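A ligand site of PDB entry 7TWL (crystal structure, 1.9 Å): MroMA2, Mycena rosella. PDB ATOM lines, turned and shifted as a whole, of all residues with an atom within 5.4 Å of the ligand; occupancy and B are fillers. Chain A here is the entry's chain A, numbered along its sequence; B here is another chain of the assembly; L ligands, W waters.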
ATOM      1  N   ILE A  19      24.737 -26.724   6.001  1.00  0.00           N
ATOM      2  CA  ILE A  19      23.328 -27.099   5.987  1.00  0.00           C
ATOM      3  C   ILE A  19      23.038 -28.041   4.819  1.00  0.00           C
ATOM      4  O   ILE A  19      22.409 -29.098   5.005  1.00  0.00           O
ATOM      5  CB  ILE A  19      22.391 -25.868   5.971  1.00  0.00           C
ATOM      6  CG1 ILE A  19      22.631 -24.920   7.160  1.00  0.00           C
ATOM      7  CG2 ILE A  19      20.929 -26.303   5.891  1.00  0.00           C
ATOM      8  CD1 ILE A  19      22.260 -25.515   8.526  1.00  0.00           C
ATOM      9  N   TYR A  99      26.002 -30.112  12.435  1.00  0.00           N
ATOM     10  CA  TYR A  99      25.498 -29.504  11.215  1.00  0.00           C
ATOM     11  C   TYR A  99      25.450 -27.974  11.343  1.00  0.00           C
ATOM     12  O   TYR A  99      25.356 -27.408  12.437  1.00  0.00           O
ATOM     13  CB  TYR A  99      24.153 -30.084  10.804  1.00  0.00           C
ATOM     14  CG  TYR A  99      22.987 -29.707  11.688  1.00  0.00           C
ATOM     15  CD1 TYR A  99      22.176 -28.638  11.356  1.00  0.00           C
ATOM     16  CD2 TYR A  99      22.662 -30.450  12.803  1.00  0.00           C
ATOM     17  CE1 TYR A  99      21.070 -28.298  12.123  1.00  0.00           C
ATOM     18  CE2 TYR A  99      21.564 -30.136  13.583  1.00  0.00           C
ATOM     19  CZ  TYR A  99      20.763 -29.055  13.245  1.00  0.00           C
ATOM     20  OH  TYR A  99      19.688 -28.714  14.004  1.00  0.00           O
ATOM     21  N   GLY A 100      25.500 -27.313  10.176  1.00  0.00           N
ATOM     22  CA  GLY A 100      25.551 -25.861  10.144  1.00  0.00           C
ATOM     23  C   GLY A 100      26.898 -25.356  10.677  1.00  0.00           C
ATOM     24  O   GLY A 100      27.938 -25.921  10.380  1.00  0.00           O
ATOM     25  N   HIS A 101      26.834 -24.283  11.472  1.00  0.00           N
ATOM     26  CA  HIS A 101      27.966 -23.773  12.242  1.00  0.00           C
ATOM     27  C   HIS A 101      27.893 -24.405  13.629  1.00  0.00           C
ATOM     28  O   HIS A 101      26.839 -24.371  14.261  1.00  0.00           O
ATOM     29  CB  HIS A 101      27.777 -22.259  12.347  1.00  0.00           C
ATOM     30  CG  HIS A 101      28.908 -21.510  12.977  1.00  0.00           C
ATOM     31  ND1 HIS A 101      29.383 -21.793  14.246  1.00  0.00           N
ATOM     32  CD2 HIS A 101      29.575 -20.411  12.543  1.00  0.00           C
ATOM     33  CE1 HIS A 101      30.348 -20.939  14.545  1.00  0.00           C
ATOM     34  NE2 HIS A 101      30.480 -20.072  13.507  1.00  0.00           N
ATOM     35  N   PRO A 102      28.984 -25.004  14.148  1.00  0.00           N
ATOM     36  CA  PRO A 102      28.893 -25.794  15.385  1.00  0.00           C
ATOM     37  C   PRO A 102      28.714 -24.952  16.645  1.00  0.00           C
ATOM     38  O   PRO A 102      28.552 -25.515  17.735  1.00  0.00           O
ATOM     39  CB  PRO A 102      30.246 -26.515  15.417  1.00  0.00           C
ATOM     40  CG  PRO A 102      31.191 -25.511  14.782  1.00  0.00           C
ATOM     41  CD  PRO A 102      30.373 -24.930  13.633  1.00  0.00           C
ATOM     42  N   VAL A 104      26.508 -22.061  16.599  1.00  0.00           N
ATOM     43  CA  VAL A 104      25.313 -21.269  16.397  1.00  0.00           C
ATOM     44  C   VAL A 104      24.112 -22.143  16.769  1.00  0.00           C
ATOM     45  O   VAL A 104      23.811 -23.104  16.050  1.00  0.00           O
ATOM     46  CB  VAL A 104      25.271 -20.724  14.942  1.00  0.00           C
ATOM     47  CG1 VAL A 104      23.962 -20.054  14.565  1.00  0.00           C
ATOM     48  CG2 VAL A 104      26.426 -19.753  14.696  1.00  0.00           C
ATOM     49  N   PHE A 105      23.460 -21.808  17.895  1.00  0.00           N
ATOM     50  CA  PHE A 105      22.344 -22.558  18.442  1.00  0.00           C
ATOM     51  C   PHE A 105      22.791 -23.976  18.742  1.00  0.00           C
ATOM     52  O   PHE A 105      22.102 -24.922  18.381  1.00  0.00           O
ATOM     53  CB  PHE A 105      21.114 -22.507  17.513  1.00  0.00           C
ATOM     54  CG  PHE A 105      20.426 -21.168  17.419  1.00  0.00           C
ATOM     55  CD1 PHE A 105      21.034 -20.106  16.767  1.00  0.00           C
ATOM     56  CD2 PHE A 105      19.165 -20.964  17.963  1.00  0.00           C
ATOM     57  CE1 PHE A 105      20.399 -18.879  16.647  1.00  0.00           C
ATOM     58  CE2 PHE A 105      18.531 -19.730  17.855  1.00  0.00           C
ATOM     59  CZ  PHE A 105      19.168 -18.680  17.233  1.00  0.00           C
ATOM     60  N   VAL A 106      23.961 -24.111  19.405  1.00  0.00           N
ATOM     61  CA  VAL A 106      24.515 -25.392  19.842  1.00  0.00           C
ATOM     62  C   VAL A 106      25.126 -25.252  21.243  1.00  0.00           C
ATOM     63  O   VAL A 106      26.096 -24.507  21.430  1.00  0.00           O
ATOM     64  CB  VAL A 106      25.592 -25.920  18.859  1.00  0.00           C
ATOM     65  CG1 VAL A 106      26.172 -27.253  19.321  1.00  0.00           C
ATOM     66  CG2 VAL A 106      25.083 -26.034  17.429  1.00  0.00           C
ATOM     67  N   ILE A 129      28.884 -23.172   7.797  1.00  0.00           N
ATOM     68  CA  ILE A 129      27.805 -22.441   7.145  1.00  0.00           C
ATOM     69  C   ILE A 129      26.543 -22.611   7.972  1.00  0.00           C
ATOM     70  O   ILE A 129      26.061 -23.744   8.106  1.00  0.00           O
ATOM     71  CB  ILE A 129      27.578 -22.986   5.715  1.00  0.00           C
ATOM     72  CG1 ILE A 129      28.828 -22.862   4.840  1.00  0.00           C
ATOM     73  CG2 ILE A 129      26.343 -22.325   5.105  1.00  0.00           C
ATOM     74  CD1 ILE A 129      29.206 -21.399   4.508  1.00  0.00           C
ATOM     75  N   SER A 130      25.987 -21.503   8.481  1.00  0.00           N
ATOM     76  CA  SER A 130      24.803 -21.537   9.327  1.00  0.00           C
ATOM     77  C   SER A 130      23.522 -21.480   8.483  1.00  0.00           C
ATOM     78  O   SER A 130      23.542 -21.121   7.306  1.00  0.00           O
ATOM     79  CB  SER A 130      24.840 -20.404  10.328  1.00  0.00           C
ATOM     80  OG  SER A 130      24.344 -19.188   9.764  1.00  0.00           O
ATOM     81  N   ALA A 131      22.385 -21.773   9.125  1.00  0.00           N
ATOM     82  CA  ALA A 131      21.078 -21.588   8.494  1.00  0.00           C
ATOM     83  C   ALA A 131      20.855 -20.128   8.123  1.00  0.00           C
ATOM     84  O   ALA A 131      20.204 -19.853   7.120  1.00  0.00           O
ATOM     85  CB  ALA A 131      19.973 -22.066   9.412  1.00  0.00           C
ATOM     86  N   GLU A 132      21.354 -19.183   8.942  1.00  0.00           N
ATOM     87  CA  GLU A 132      21.260 -17.757   8.586  1.00  0.00           C
ATOM     88  C   GLU A 132      22.090 -17.433   7.338  1.00  0.00           C
ATOM     89  O   GLU A 132      21.639 -16.679   6.478  1.00  0.00           O
ATOM     90  CB  GLU A 132      21.667 -16.868   9.762  1.00  0.00           C
ATOM     91  CG  GLU A 132      20.487 -16.185  10.382  1.00  0.00           C
ATOM     92  CD  GLU A 132      20.866 -15.287  11.538  1.00  0.00           C
ATOM     93  OE1 GLU A 132      22.023 -14.777  11.546  1.00  0.00           O
ATOM     94  OE2 GLU A 132      20.018 -15.091  12.427  1.00  0.00           O
ATOM     95  N   TYR A 134      22.692 -19.494   4.909  1.00  0.00           N
ATOM     96  CA  TYR A 134      21.903 -20.073   3.823  1.00  0.00           C
ATOM     97  C   TYR A 134      20.741 -19.142   3.491  1.00  0.00           C
ATOM     98  O   TYR A 134      20.462 -18.892   2.315  1.00  0.00           O
ATOM     99  CB  TYR A 134      21.446 -21.488   4.242  1.00  0.00           C
ATOM    100  CG  TYR A 134      21.296 -22.535   3.171  1.00  0.00           C
ATOM    101  CD1 TYR A 134      21.573 -22.280   1.821  1.00  0.00           C
ATOM    102  CD2 TYR A 134      20.870 -23.814   3.501  1.00  0.00           C
ATOM    103  CE1 TYR A 134      21.425 -23.269   0.855  1.00  0.00           C
ATOM    104  CE2 TYR A 134      20.732 -24.808   2.545  1.00  0.00           C
ATOM    105  CZ  TYR A 134      21.000 -24.536   1.210  1.00  0.00           C
ATOM    106  OH  TYR A 134      20.871 -25.527   0.276  1.00  0.00           O
ATOM    107  N   ILE A 171      13.927 -15.485  13.286  1.00  0.00           N
ATOM    108  CA  ILE A 171      13.442 -16.206  14.454  1.00  0.00           C
ATOM    109  C   ILE A 171      13.645 -17.690  14.201  1.00  0.00           C
ATOM    110  O   ILE A 171      13.066 -18.238  13.263  1.00  0.00           O
ATOM    111  CB  ILE A 171      11.962 -15.891  14.783  1.00  0.00           C
ATOM    112  CG1 ILE A 171      11.646 -14.382  14.743  1.00  0.00           C
ATOM    113  CG2 ILE A 171      11.600 -16.511  16.130  1.00  0.00           C
ATOM    114  CD1 ILE A 171      10.173 -14.008  14.966  1.00  0.00           C
ATOM    115  N   TRP A 172      14.465 -18.336  15.051  1.00  0.00           N
ATOM    116  CA  TRP A 172      14.896 -19.707  14.890  1.00  0.00           C
ATOM    117  C   TRP A 172      14.092 -20.611  15.821  1.00  0.00           C
ATOM    118  O   TRP A 172      13.550 -20.149  16.837  1.00  0.00           O
ATOM    119  CB  TRP A 172      16.391 -19.866  15.231  1.00  0.00           C
ATOM    120  CG  TRP A 172      17.434 -19.067  14.497  1.00  0.00           C
ATOM    121  CD1 TRP A 172      17.521 -17.704  14.350  1.00  0.00           C
ATOM    122  CD2 TRP A 172      18.623 -19.605  13.886  1.00  0.00           C
ATOM    123  NE1 TRP A 172      18.672 -17.370  13.649  1.00  0.00           N
ATOM    124  CE2 TRP A 172      19.361 -18.519  13.354  1.00  0.00           C
ATOM    125  CE3 TRP A 172      19.110 -20.903  13.689  1.00  0.00           C
ATOM    126  CZ2 TRP A 172      20.576 -18.693  12.702  1.00  0.00           C
ATOM    127  CZ3 TRP A 172      20.314 -21.080  13.046  1.00  0.00           C
ATOM    128  CH2 TRP A 172      21.022 -19.986  12.526  1.00  0.00           C
ATOM    129  N   GLN A 173      14.069 -21.908  15.496  1.00  0.00           N
ATOM    130  CA  GLN A 173      13.381 -22.916  16.311  1.00  0.00           C
ATOM    131  C   GLN A 173      11.905 -22.581  16.552  1.00  0.00           C
ATOM    132  O   GLN A 173      11.373 -22.834  17.637  1.00  0.00           O
ATOM    133  CB  GLN A 173      14.167 -23.186  17.609  1.00  0.00           C
ATOM    134  CG  GLN A 173      15.596 -23.629  17.350  1.00  0.00           C
ATOM    135  CD  GLN A 173      16.213 -24.528  18.411  1.00  0.00           C
ATOM    136  OE1 GLN A 173      16.011 -24.333  19.614  1.00  0.00           O
ATOM    137  NE2 GLN A 173      16.989 -25.490  17.962  1.00  0.00           N
ATOM    138  N   VAL A 174      11.221 -22.061  15.525  1.00  0.00           N
ATOM    139  CA  VAL A 174       9.821 -21.670  15.651  1.00  0.00           C
ATOM    140  C   VAL A 174       8.940 -22.912  15.836  1.00  0.00           C
ATOM    141  O   VAL A 174       7.805 -22.787  16.315  1.00  0.00           O
ATOM    142  CB  VAL A 174       9.355 -20.808  14.457  1.00  0.00           C
ATOM    143  CG1 VAL A 174      10.130 -19.489  14.347  1.00  0.00           C
ATOM    144  CG2 VAL A 174       9.371 -21.555  13.138  1.00  0.00           C
ATOM    145  N   TYR A 209      11.195 -20.146   5.963  1.00  0.00           N
ATOM    146  CA  TYR A 209      12.394 -20.566   5.256  1.00  0.00           C
ATOM    147  C   TYR A 209      12.851 -21.942   5.709  1.00  0.00           C
ATOM    148  O   TYR A 209      13.070 -22.175   6.910  1.00  0.00           O
ATOM    149  CB  TYR A 209      13.550 -19.574   5.495  1.00  0.00           C
ATOM    150  CG  TYR A 209      14.856 -20.019   4.901  1.00  0.00           C
ATOM    151  CD1 TYR A 209      14.969 -20.247   3.534  1.00  0.00           C
ATOM    152  CD2 TYR A 209      15.975 -20.260   5.694  1.00  0.00           C
ATOM    153  CE1 TYR A 209      16.165 -20.666   2.976  1.00  0.00           C
ATOM    154  CE2 TYR A 209      17.181 -20.674   5.149  1.00  0.00           C
ATOM    155  CZ  TYR A 209      17.279 -20.843   3.770  1.00  0.00           C
ATOM    156  OH  TYR A 209      18.453 -21.292   3.242  1.00  0.00           O
ATOM    157  N   ILE A 210      12.979 -22.861   4.738  1.00  0.00           N
ATOM    158  CA  ILE A 210      13.711 -24.110   4.929  1.00  0.00           C
ATOM    159  C   ILE A 210      14.688 -24.254   3.779  1.00  0.00           C
ATOM    160  O   ILE A 210      14.291 -24.551   2.639  1.00  0.00           O
ATOM    161  CB  ILE A 210      12.790 -25.352   5.091  1.00  0.00           C
ATOM    162  CG1 ILE A 210      11.860 -25.234   6.309  1.00  0.00           C
ATOM    163  CG2 ILE A 210      13.632 -26.622   5.206  1.00  0.00           C
ATOM    164  CD1 ILE A 210      10.680 -26.218   6.294  1.00  0.00           C
ATOM    165  N   GLY A 211      15.980 -24.037   4.082  1.00  0.00           N
ATOM    166  CA  GLY A 211      17.019 -24.251   3.090  1.00  0.00           C
ATOM    167  C   GLY A 211      17.117 -25.725   2.676  1.00  0.00           C
ATOM    168  O   GLY A 211      16.948 -26.605   3.518  1.00  0.00           O
ATOM    169  N   ALA A 212      17.437 -25.987   1.402  1.00  0.00           N
ATOM    170  CA  ALA A 212      17.456 -27.334   0.849  1.00  0.00           C
ATOM    171  C   ALA A 212      18.609 -28.170   1.426  1.00  0.00           C
ATOM    172  O   ALA A 212      19.770 -27.800   1.289  1.00  0.00           O
ATOM    173  CB  ALA A 212      17.562 -27.286  -0.667  1.00  0.00           C
ATOM    174  N   ILE A 213      18.276 -29.323   2.048  1.00  0.00           N
ATOM    175  CA  ILE A 213      19.299 -30.148   2.676  1.00  0.00           C
ATOM    176  C   ILE A 213      19.842 -31.152   1.662  1.00  0.00           C
ATOM    177  O   ILE A 213      21.054 -31.348   1.553  1.00  0.00           O
ATOM    178  CB  ILE A 213      18.773 -30.829   3.952  1.00  0.00           C
ATOM    179  CG1 ILE A 213      18.270 -29.815   4.992  1.00  0.00           C
ATOM    180  CG2 ILE A 213      19.852 -31.730   4.545  1.00  0.00           C
ATOM    181  CD1 ILE A 213      17.383 -30.427   6.043  1.00  0.00           C
ATOM    182  N   THR A 240      10.709 -28.694  12.916  1.00  0.00           N
ATOM    183  CA  THR A 240      11.876 -28.384  13.734  1.00  0.00           C
ATOM    184  C   THR A 240      12.990 -27.762  12.888  1.00  0.00           C
ATOM    185  O   THR A 240      13.957 -27.229  13.436  1.00  0.00           O
ATOM    186  CB  THR A 240      12.356 -29.621  14.512  1.00  0.00           C
ATOM    187  OG1 THR A 240      12.557 -30.640  13.540  1.00  0.00           O
ATOM    188  CG2 THR A 240      11.350 -30.078  15.536  1.00  0.00           C
ATOM    189  N   THR A 241      12.825 -27.797  11.565  1.00  0.00           N
ATOM    190  CA  THR A 241      13.797 -27.206  10.649  1.00  0.00           C
ATOM    191  C   THR A 241      13.443 -25.756  10.300  1.00  0.00           C
ATOM    192  O   THR A 241      14.316 -25.032   9.808  1.00  0.00           O
ATOM    193  CB  THR A 241      13.956 -28.066   9.381  1.00  0.00           C
ATOM    194  OG1 THR A 241      14.165 -29.427   9.743  1.00  0.00           O
ATOM    195  CG2 THR A 241      15.143 -27.681   8.530  1.00  0.00           C
ATOM    196  N   SER A 242      12.195 -25.326  10.532  1.00  0.00           N
ATOM    197  CA  SER A 242      11.693 -24.023  10.083  1.00  0.00           C
ATOM    198  C   SER A 242      12.401 -22.846  10.780  1.00  0.00           C
ATOM    199  O   SER A 242      12.585 -22.858  11.992  1.00  0.00           O
ATOM    200  CB  SER A 242      10.202 -23.911  10.298  1.00  0.00           C
ATOM    201  OG  SER A 242       9.511 -24.976   9.642  1.00  0.00           O
ATOM    202  N   THR A 243      12.739 -21.820   9.976  1.00  0.00           N
ATOM    203  CA  THR A 243      13.190 -20.517  10.450  1.00  0.00           C
ATOM    204  C   THR A 243      12.284 -19.441   9.841  1.00  0.00           C
ATOM    205  O   THR A 243      11.815 -19.613   8.721  1.00  0.00           O
ATOM    206  CB  THR A 243      14.676 -20.287  10.110  1.00  0.00           C
ATOM    207  OG1 THR A 243      15.476 -21.284  10.753  1.00  0.00           O
ATOM    208  CG2 THR A 243      15.202 -18.929  10.533  1.00  0.00           C
ATOM    209  N   LEU B 392      14.919 -33.393  12.349  1.00  0.00           N
ATOM    210  CA  LEU B 392      16.067 -32.494  12.703  1.00  0.00           C
ATOM    211  C   LEU B 392      16.419 -32.592  14.190  1.00  0.00           C
ATOM    212  O   LEU B 392      15.572 -32.395  15.047  1.00  0.00           O
ATOM    213  CB  LEU B 392      15.734 -31.042  12.315  1.00  0.00           C
ATOM    214  CG  LEU B 392      16.906 -30.198  11.792  1.00  0.00           C
ATOM    215  CD1 LEU B 392      16.806 -28.749  12.219  1.00  0.00           C
ATOM    216  CD2 LEU B 392      18.240 -30.778  12.213  1.00  0.00           C
ATOM    217  N   ALA B 393      17.697 -32.877  14.477  1.00  0.00           N
ATOM    218  CA  ALA B 393      18.265 -32.798  15.813  1.00  0.00           C
ATOM    219  C   ALA B 393      18.285 -31.348  16.309  1.00  0.00           C
ATOM    220  O   ALA B 393      19.005 -30.511  15.764  1.00  0.00           O
ATOM    221  CB  ALA B 393      19.648 -33.390  15.807  1.00  0.00           C
ATOM    222  N   MLE B 394      17.553 -31.004  17.392  1.00  0.00           N
ATOM    223  CN  MLE B 394      16.692 -31.936  18.109  1.00  0.00           C
ATOM    224  CA  MLE B 394      17.716 -29.639  17.949  1.00  0.00           C
ATOM    225  CB  MLE B 394      16.450 -29.039  18.578  1.00  0.00           C
ATOM    226  CG  MLE B 394      15.262 -28.971  17.625  1.00  0.00           C
ATOM    227  CD1 MLE B 394      14.054 -28.383  18.337  1.00  0.00           C
ATOM    228  CD2 MLE B 394      15.597 -28.125  16.398  1.00  0.00           C
ATOM    229  C   MLE B 394      18.878 -29.642  18.933  1.00  0.00           C
ATOM    230  O   MLE B 394      18.957 -30.570  19.748  1.00  0.00           O
ATOM    231  N   MVA B 395      19.856 -28.718  18.822  1.00  0.00           N
ATOM    232  CN  MVA B 395      19.764 -27.554  17.941  1.00  0.00           C
ATOM    233  CA  MVA B 395      21.101 -28.882  19.616  1.00  0.00           C
ATOM    234  CB  MVA B 395      22.363 -29.162  18.771  1.00  0.00           C
ATOM    235  CG1 MVA B 395      23.371 -30.007  19.550  1.00  0.00           C
ATOM    236  CG2 MVA B 395      22.083 -29.848  17.448  1.00  0.00           C
ATOM    237  C   MVA B 395      21.278 -27.753  20.632  1.00  0.00           C
ATOM    238  O   MVA B 395      22.374 -27.535  21.150  1.00  0.00           O
ATOM    239  N   VAL B 396      20.208 -27.025  20.954  1.00  0.00           N
ATOM    240  CA  VAL B 396      20.200 -26.066  22.094  1.00  0.00           C
ATOM    241  C   VAL B 396      18.803 -26.065  22.698  1.00  0.00           C
ATOM    242  O   VAL B 396      17.823 -26.393  22.020  1.00  0.00           O
ATOM    243  CB  VAL B 396      20.667 -24.655  21.652  1.00  0.00           C
ATOM    244  CG1 VAL B 396      19.612 -23.917  20.855  1.00  0.00           C
ATOM    245  CG2 VAL B 396      21.142 -23.802  22.829  1.00  0.00           C
HETATM  246  N1  LIG L   1      23.949 -25.030  14.134  1.00  0.00           N
HETATM  247  C1  LIG L   1      22.825 -24.913  13.181  1.00  0.00           C
HETATM  248  C2  LIG L   1      21.508 -24.586  13.903  1.00  0.00           C
HETATM  249  C3  LIG L   1      21.075 -25.597  14.983  1.00  0.00           C
HETATM  250  S1  LIG L   1      19.536 -25.112  15.835  1.00  0.00           S
HETATM  251  C4  LIG L   1      23.155 -23.773  12.204  1.00  0.00           C
HETATM  252  O1  LIG L   1      22.307 -23.363  11.429  1.00  0.00           O
HETATM  253  O2  LIG L   1      24.275 -23.228  12.180  1.00  0.00           O
HETATM  254  C5  LIG L   1      18.247 -25.694  14.694  1.00  0.00           C
HETATM  255  C6  LIG L   1      17.549 -24.524  14.053  1.00  0.00           C
HETATM  256  O3  LIG L   1      18.359 -24.029  12.958  1.00  0.00           O
HETATM  257  C7  LIG L   1      16.208 -24.846  13.392  1.00  0.00           C
HETATM  258  O4  LIG L   1      15.132 -24.891  14.314  1.00  0.00           O
HETATM  259  C8  LIG L   1      16.089 -23.660  12.422  1.00  0.00           C
HETATM  260  O5  LIG L   1      15.670 -22.445  12.996  1.00  0.00           O
HETATM  261  C9  LIG L   1      17.529 -23.589  11.908  1.00  0.00           C
HETATM  262  N2  LIG L   1      17.715 -24.442  10.739  1.00  0.00           N
HETATM  263  C10 LIG L   1      18.366 -25.643  10.690  1.00  0.00           C
HETATM  264  N3  LIG L   1      18.353 -26.191   9.502  1.00  0.00           N
HETATM  265  C11 LIG L   1      17.639 -25.300   8.720  1.00  0.00           C
HETATM  266  C12 LIG L   1      17.276 -25.320   7.361  1.00  0.00           C
HETATM  267  N4  LIG L   1      17.595 -26.325   6.538  1.00  0.00           N
HETATM  268  N5  LIG L   1      16.587 -24.258   6.873  1.00  0.00           N
HETATM  269  C13 LIG L   1      16.246 -23.271   7.721  1.00  0.00           C
HETATM  270  N6  LIG L   1      16.527 -23.161   9.023  1.00  0.00           N
HETATM  271  C14 LIG L   1      17.247 -24.210   9.464  1.00  0.00           C
HETATM  272  O   HOH W   1      11.772 -24.637  13.815  1.00  0.00           O
HETATM  273  O   HOH W   2      18.854 -28.610   8.290  1.00  0.00           O
HETATM  274  O   HOH W   3      12.553 -26.231  16.221  1.00  0.00           O
HETATM  275  O   HOH W   4      23.956 -27.947  14.729  1.00  0.00           O
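O of His 101 lies within hydrogen-bond range of N1 of the ligand (3.0 Å).
O of Val 104 is in hydrogen-bond range of N1 of the ligand, 2.7 Å away.
The backbone carbonyl oxygen (O) of Gly 211 is in hydrogen-bond range of a nitrogen (N4) of the ligand (3.1 Å).
O of Ser 242 sits at hydrogen-bond distance from O5 of the ligand, 3.3 Å away.
An oxygen (O5) of the ligand is in hydrogen-bond range of the side-chain hydroxyl of Thr 243 (2.5 Å).
The backbone carbonyl oxygen (O) of Tyr 99 sits at hydrogen-bond distance from a nitrogen (N1) of the ligand (3.2 Å).
The side-chain amide nitrogen (NE2) of Gln 173 lies close to a sulfur (S1) of the ligand, 3.3 Å away.
O1 of the ligand lies within hydrogen-bond range of N of Ala 131 (2.8 Å).
N of His 101 is in hydrogen-bond range of O2 of the ligand.
An oxygen (O5) of the ligand sits at hydrogen-bond distance from the backbone NH (N) of Gln 173 (3.0 Å).
The backbone carbonyl oxygen (O) of Thr 240 sits at hydrogen-bond distance from an oxygen (O4) of the ligand, at 2.8 Å.
The backbone NH (N) of Gly 211 lies within hydrogen-bond range of a nitrogen (N5) of the ligand.
OH of Tyr 99 is in hydrogen-bond range of O of Ala 393 of chain B.
The side-chain hydroxyl of Ser 130 sits at hydrogen-bond distance from the backbone NH of Glu 132 (3.1 Å).
The backbone carbonyl oxygen (O) of Thr 243 is in hydrogen-bond range of the backbone NH (N) of Tyr 209 (2.9 Å).
The backbone carbonyl oxygen of Tyr 134 sits close to the side-chain hydroxyl of Tyr 209.
O of Ile 129 lies within hydrogen-bond range of N of His 101, at 3.5 Å.
The indole nitrogen (NE1) of Trp 172 sits at hydrogen-bond distance from the side-chain carboxylate (OE2) of Glu 132, at 2.9 Å.
The backbone carbonyl oxygen (O) of Phe 105 sits close to a sulfur (S1) of the ligand (3.6 Å).
The backbone carbonyl oxygen (O) of Thr 241 sits close to a nitrogen (N6) of the ligand (3.0 Å).
Ile 19 touches the ligand (CG2 to N4, 3.4 Å).
CA of Gly 100 touches O2 of the ligand, 3.6 Å away.
CG2 of Val 106 touches N1 of the ligand, at 3.6 Å.
Ser 130 touches the ligand.
CE3 of Trp 172 touches O3 of the ligand, at 3.3 Å.
Tyr 209 touches the ligand.
Ile 210 touches the ligand.
Ile 213 touches the ligand (CG1 to N4, 3.9 Å).
CD1 of Leu 392 of chain B touches C10 of the ligand, at 3.8 Å.
CD2 of MLE 394 of chain B touches O4 of the ligand, 3.9 Å away.
MVA 395 of chain B touches the ligand (CN to S1, 3.2 Å).
Hydrophobic or aromatic side chains that line the ligand: Ile 19, Tyr 99, His 101, Val 104, Phe 105, Val 106, Ala 131, Trp 172, Tyr 209, Ile 213 and Leu 392 of chain B.
The nearest printed residue that does not touch the ligand is Ile 129 (4.5 Å).
Water W4 bridges the backbone carbonyl oxygen of Tyr 99 (2.7 Å) and a nitrogen (N1) of the ligand (3.0 Å).
Water W1 lies within hydrogen-bond range of O of Ser 242 (2.7 Å), N of Val 174 (3.1 Å), O4 of the ligand (3.4 Å) and O of Thr 240 (3.4 Å).
Water W3 bridges the backbone carbonyl oxygen of Thr 240 (3.3 Å) and an oxygen (O4) of the ligand (3.5 Å).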
